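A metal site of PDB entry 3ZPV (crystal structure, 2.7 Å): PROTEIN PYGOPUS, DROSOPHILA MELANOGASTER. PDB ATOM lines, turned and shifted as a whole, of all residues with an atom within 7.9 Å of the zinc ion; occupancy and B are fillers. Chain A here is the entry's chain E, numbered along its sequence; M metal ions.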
ATOM      1  N   PRO A   7      -8.766 -18.107 -32.614  1.00  0.00           N
ATOM      2  CA  PRO A   7      -7.533 -17.372 -32.538  1.00  0.00           C
ATOM      3  C   PRO A   7      -7.711 -15.845 -32.394  1.00  0.00           C
ATOM      4  O   PRO A   7      -8.617 -15.252 -32.966  1.00  0.00           O
ATOM      5  CB  PRO A   7      -6.862 -17.726 -33.855  1.00  0.00           C
ATOM      6  CG  PRO A   7      -7.989 -17.885 -34.795  1.00  0.00           C
ATOM      7  CD  PRO A   7      -9.148 -18.371 -34.001  1.00  0.00           C
ATOM      8  N   CYS A   8      -6.798 -15.231 -31.640  1.00  0.00           N
ATOM      9  CA  CYS A   8      -6.689 -13.784 -31.518  1.00  0.00           C
ATOM     10  C   CYS A   8      -6.416 -13.173 -32.873  1.00  0.00           C
ATOM     11  O   CYS A   8      -5.618 -13.694 -33.630  1.00  0.00           O
ATOM     12  CB  CYS A   8      -5.528 -13.438 -30.551  1.00  0.00           C
ATOM     13  SG  CYS A   8      -5.132 -11.680 -30.339  1.00  0.00           S
ATOM     14  N   GLY A   9      -7.090 -12.098 -33.196  1.00  0.00           N
ATOM     15  CA  GLY A   9      -6.895 -11.439 -34.485  1.00  0.00           C
ATOM     16  C   GLY A   9      -5.552 -10.759 -34.660  1.00  0.00           C
ATOM     17  O   GLY A   9      -5.182 -10.436 -35.768  1.00  0.00           O
ATOM     18  N   MET A  10      -4.831 -10.533 -33.561  1.00  0.00           N
ATOM     19  CA  MET A  10      -3.506  -9.940 -33.547  1.00  0.00           C
ATOM     20  C   MET A  10      -2.436 -11.023 -33.570  1.00  0.00           C
ATOM     21  O   MET A  10      -1.704 -11.147 -34.536  1.00  0.00           O
ATOM     22  CB  MET A  10      -3.324  -9.070 -32.272  1.00  0.00           C
ATOM     23  CG  MET A  10      -3.618  -7.596 -32.465  1.00  0.00           C
ATOM     24  SD  MET A  10      -2.527  -6.751 -33.627  1.00  0.00           S
ATOM     25  CE  MET A  10      -0.875  -7.214 -33.041  1.00  0.00           C
ATOM     26  N   CYS A  11      -2.365 -11.807 -32.503  1.00  0.00           N
ATOM     27  CA  CYS A  11      -1.263 -12.750 -32.312  1.00  0.00           C
ATOM     28  C   CYS A  11      -1.528 -14.149 -32.853  1.00  0.00           C
ATOM     29  O   CYS A  11      -0.625 -14.973 -32.902  1.00  0.00           O
ATOM     30  CB  CYS A  11      -0.902 -12.831 -30.818  1.00  0.00           C
ATOM     31  SG  CYS A  11      -2.037 -13.771 -29.775  1.00  0.00           S
ATOM     32  N   HIS A  12      -2.777 -14.432 -33.223  1.00  0.00           N
ATOM     33  CA  HIS A  12      -3.185 -15.701 -33.832  1.00  0.00           C
ATOM     34  C   HIS A  12      -3.084 -16.890 -32.914  1.00  0.00           C
ATOM     35  O   HIS A  12      -3.247 -18.010 -33.356  1.00  0.00           O
ATOM     36  CB  HIS A  12      -2.388 -15.981 -35.102  1.00  0.00           C
ATOM     37  CG  HIS A  12      -2.357 -14.807 -36.042  1.00  0.00           C
ATOM     38  ND1 HIS A  12      -3.504 -14.287 -36.594  1.00  0.00           N
ATOM     39  CD2 HIS A  12      -1.327 -14.037 -36.471  1.00  0.00           C
ATOM     40  CE1 HIS A  12      -3.176 -13.251 -37.355  1.00  0.00           C
ATOM     41  NE2 HIS A  12      -1.862 -13.082 -37.291  1.00  0.00           N
ATOM     42  N   LYS A  13      -2.855 -16.657 -31.624  1.00  0.00           N
ATOM     43  CA  LYS A  13      -2.902 -17.727 -30.653  1.00  0.00           C
ATOM     44  C   LYS A  13      -4.267 -17.850 -30.034  1.00  0.00           C
ATOM     45  O   LYS A  13      -5.107 -16.988 -30.134  1.00  0.00           O
ATOM     46  CB  LYS A  13      -1.866 -17.510 -29.567  1.00  0.00           C
ATOM     47  CG  LYS A  13      -0.445 -17.596 -30.068  1.00  0.00           C
ATOM     48  CD  LYS A  13       0.516 -17.013 -29.066  1.00  0.00           C
ATOM     49  CE  LYS A  13       1.935 -17.490 -29.336  1.00  0.00           C
ATOM     50  NZ  LYS A  13       2.875 -17.018 -28.285  1.00  0.00           N
ATOM     51  N   GLU A  14      -4.476 -18.994 -29.390  1.00  0.00           N
ATOM     52  CA  GLU A  14      -5.758 -19.331 -28.787  1.00  0.00           C
ATOM     53  C   GLU A  14      -6.245 -18.267 -27.819  1.00  0.00           C
ATOM     54  O   GLU A  14      -5.454 -17.758 -27.017  1.00  0.00           O
ATOM     55  CB  GLU A  14      -5.580 -20.642 -28.029  1.00  0.00           C
ATOM     56  CG  GLU A  14      -6.879 -21.264 -27.587  1.00  0.00           C
ATOM     57  CD  GLU A  14      -6.697 -22.516 -26.755  1.00  0.00           C
ATOM     58  OE1 GLU A  14      -5.590 -23.103 -26.767  1.00  0.00           O
ATOM     59  OE2 GLU A  14      -7.699 -22.925 -26.102  1.00  0.00           O
ATOM     60  N   VAL A  15      -7.527 -17.924 -27.897  1.00  0.00           N
ATOM     61  CA  VAL A  15      -8.223 -17.179 -26.874  1.00  0.00           C
ATOM     62  C   VAL A  15      -9.102 -18.141 -26.110  1.00  0.00           C
ATOM     63  O   VAL A  15     -10.053 -18.637 -26.658  1.00  0.00           O
ATOM     64  CB  VAL A  15      -9.136 -16.114 -27.475  1.00  0.00           C
ATOM     65  CG1 VAL A  15      -9.966 -15.427 -26.392  1.00  0.00           C
ATOM     66  CG2 VAL A  15      -8.328 -15.073 -28.217  1.00  0.00           C
ATOM     67  N   ASP A  19      -8.717 -16.238 -20.567  1.00  0.00           N
ATOM     68  CA  ASP A  19      -8.051 -15.088 -21.116  1.00  0.00           C
ATOM     69  C   ASP A  19      -8.946 -13.861 -20.901  1.00  0.00           C
ATOM     70  O   ASP A  19     -10.167 -13.984 -20.842  1.00  0.00           O
ATOM     71  CB  ASP A  19      -7.709 -15.320 -22.603  1.00  0.00           C
ATOM     72  CG  ASP A  19      -6.487 -16.210 -22.814  1.00  0.00           C
ATOM     73  OD1 ASP A  19      -5.621 -16.280 -21.904  1.00  0.00           O
ATOM     74  OD2 ASP A  19      -6.357 -16.828 -23.880  1.00  0.00           O
ATOM     75  N   GLU A  20      -8.339 -12.696 -20.772  1.00  0.00           N
ATOM     76  CA  GLU A  20      -9.057 -11.460 -20.752  1.00  0.00           C
ATOM     77  C   GLU A  20      -9.149 -11.024 -22.200  1.00  0.00           C
ATOM     78  O   GLU A  20      -8.126 -10.722 -22.811  1.00  0.00           O
ATOM     79  CB  GLU A  20      -8.306 -10.396 -19.957  1.00  0.00           C
ATOM     80  CG  GLU A  20      -8.183 -10.673 -18.475  1.00  0.00           C
ATOM     81  CD  GLU A  20      -7.648  -9.484 -17.684  1.00  0.00           C
ATOM     82  OE1 GLU A  20      -6.919  -8.607 -18.204  1.00  0.00           O
ATOM     83  OE2 GLU A  20      -7.975  -9.407 -16.486  1.00  0.00           O
ATOM     84  N   PHE A  31     -12.078 -12.731 -32.054  1.00  0.00           N
ATOM     85  CA  PHE A  31     -11.740 -12.456 -30.693  1.00  0.00           C
ATOM     86  C   PHE A  31     -10.344 -11.921 -30.654  1.00  0.00           C
ATOM     87  O   PHE A  31      -9.539 -12.204 -31.545  1.00  0.00           O
ATOM     88  CB  PHE A  31     -11.825 -13.734 -29.876  1.00  0.00           C
ATOM     89  CG  PHE A  31     -13.215 -14.218 -29.649  1.00  0.00           C
ATOM     90  CD1 PHE A  31     -13.985 -13.698 -28.618  1.00  0.00           C
ATOM     91  CD2 PHE A  31     -13.758 -15.201 -30.455  1.00  0.00           C
ATOM     92  CE1 PHE A  31     -15.254 -14.140 -28.403  1.00  0.00           C
ATOM     93  CE2 PHE A  31     -15.035 -15.653 -30.243  1.00  0.00           C
ATOM     94  CZ  PHE A  31     -15.789 -15.116 -29.218  1.00  0.00           C
ATOM     95  N   PHE A  32     -10.026 -11.176 -29.598  1.00  0.00           N
ATOM     96  CA  PHE A  32      -8.676 -10.650 -29.368  1.00  0.00           C
ATOM     97  C   PHE A  32      -8.339 -10.691 -27.894  1.00  0.00           C
ATOM     98  O   PHE A  32      -9.209 -10.454 -27.064  1.00  0.00           O
ATOM     99  CB  PHE A  32      -8.602  -9.185 -29.756  1.00  0.00           C
ATOM    100  CG  PHE A  32      -8.857  -8.899 -31.200  1.00  0.00           C
ATOM    101  CD1 PHE A  32     -10.132  -8.811 -31.684  1.00  0.00           C
ATOM    102  CD2 PHE A  32      -7.782  -8.647 -32.070  1.00  0.00           C
ATOM    103  CE1 PHE A  32     -10.356  -8.529 -33.036  1.00  0.00           C
ATOM    104  CE2 PHE A  32      -7.994  -8.342 -33.407  1.00  0.00           C
ATOM    105  CZ  PHE A  32      -9.275  -8.286 -33.898  1.00  0.00           C
ATOM    106  N   HIS A  33      -7.067 -10.950 -27.562  1.00  0.00           N
ATOM    107  CA  HIS A  33      -6.607 -10.758 -26.207  1.00  0.00           C
ATOM    108  C   HIS A  33      -6.595  -9.256 -25.916  1.00  0.00           C
ATOM    109  O   HIS A  33      -6.180  -8.461 -26.761  1.00  0.00           O
ATOM    110  CB  HIS A  33      -5.183 -11.288 -26.042  1.00  0.00           C
ATOM    111  CG  HIS A  33      -5.065 -12.757 -26.242  1.00  0.00           C
ATOM    112  ND1 HIS A  33      -4.397 -13.303 -27.319  1.00  0.00           N
ATOM    113  CD2 HIS A  33      -5.492 -13.803 -25.501  1.00  0.00           C
ATOM    114  CE1 HIS A  33      -4.410 -14.620 -27.227  1.00  0.00           C
ATOM    115  NE2 HIS A  33      -5.073 -14.954 -26.134  1.00  0.00           N
ATOM    116  N   ARG A  34      -6.974  -8.875 -24.697  1.00  0.00           N
ATOM    117  CA  ARG A  34      -6.980  -7.417 -24.298  1.00  0.00           C
ATOM    118  C   ARG A  34      -5.595  -6.799 -24.444  1.00  0.00           C
ATOM    119  O   ARG A  34      -5.469  -5.724 -24.996  1.00  0.00           O
ATOM    120  CB  ARG A  34      -7.547  -7.189 -22.881  1.00  0.00           C
ATOM    121  CG  ARG A  34      -6.716  -6.536 -21.796  1.00  0.00           C
ATOM    122  CD  ARG A  34      -7.437  -6.118 -20.596  1.00  0.00           C
ATOM    123  NE  ARG A  34      -6.420  -6.529 -19.669  1.00  0.00           N
ATOM    124  CZ  ARG A  34      -5.274  -5.901 -19.492  1.00  0.00           C
ATOM    125  NH1 ARG A  34      -4.995  -4.747 -20.096  1.00  0.00           N
ATOM    126  NH2 ARG A  34      -4.408  -6.450 -18.675  1.00  0.00           N
ATOM    127  N   THR A  35      -4.588  -7.525 -23.930  1.00  0.00           N
ATOM    128  CA  THR A  35      -3.152  -7.157 -23.999  1.00  0.00           C
ATOM    129  C   THR A  35      -2.686  -6.924 -25.423  1.00  0.00           C
ATOM    130  O   THR A  35      -2.055  -5.930 -25.691  1.00  0.00           O
ATOM    131  CB  THR A  35      -2.140  -8.168 -23.284  1.00  0.00           C
ATOM    132  OG1 THR A  35      -2.257  -9.524 -23.724  1.00  0.00           O
ATOM    133  CG2 THR A  35      -2.203  -8.159 -21.722  1.00  0.00           C
ATOM    134  N   CYS A  36      -3.049  -7.791 -26.366  1.00  0.00           N
ATOM    135  CA  CYS A  36      -2.627  -7.653 -27.777  1.00  0.00           C
ATOM    136  C   CYS A  36      -3.121  -6.406 -28.484  1.00  0.00           C
ATOM    137  O   CYS A  36      -2.514  -5.970 -29.446  1.00  0.00           O
ATOM    138  CB  CYS A  36      -3.067  -8.897 -28.606  1.00  0.00           C
ATOM    139  SG  CYS A  36      -2.262 -10.455 -28.137  1.00  0.00           S
ATOM    140  N   VAL A  37      -4.253  -5.864 -28.065  1.00  0.00           N
ATOM    141  CA  VAL A  37      -4.837  -4.717 -28.767  1.00  0.00           C
ATOM    142  C   VAL A  37      -4.538  -3.373 -28.086  1.00  0.00           C
ATOM    143  O   VAL A  37      -4.841  -2.323 -28.624  1.00  0.00           O
ATOM    144  CB  VAL A  37      -6.344  -4.874 -28.989  1.00  0.00           C
ATOM    145  CG1 VAL A  37      -6.606  -6.047 -29.887  1.00  0.00           C
ATOM    146  CG2 VAL A  37      -7.097  -5.068 -27.673  1.00  0.00           C
HETATM  147 ZN    ZN M   1      -3.526 -12.313 -28.841  1.00  0.00          ZN
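The zinc ion is bound by a ring nitrogen (ND1) of His 33, the side-chain sulfur of Cys 11, the side-chain sulfur of Cys 8 and the side-chain sulfur of Cys 36.
Of the 18 residues printed, 4 come within 4 Å of the zinc ion.
A ring nitrogen (NE2) of His 33 lies within hydrogen-bond range of the backbone carbonyl oxygen (O) of Glu 14, 3.0 Å away.
N of Cys 8 is in hydrogen-bond range of O of Lys 13, at 2.9 Å.
SG of Cys 8 sits close to N of Met 10 (3.4 Å).
The side-chain carboxylate (OD2) of Asp 19 sits at hydrogen-bond distance from a ring nitrogen (NE2) of His 33 (3.2 Å).
SG of Cys 11 lies close to N of Lys 13 (3.5 Å).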
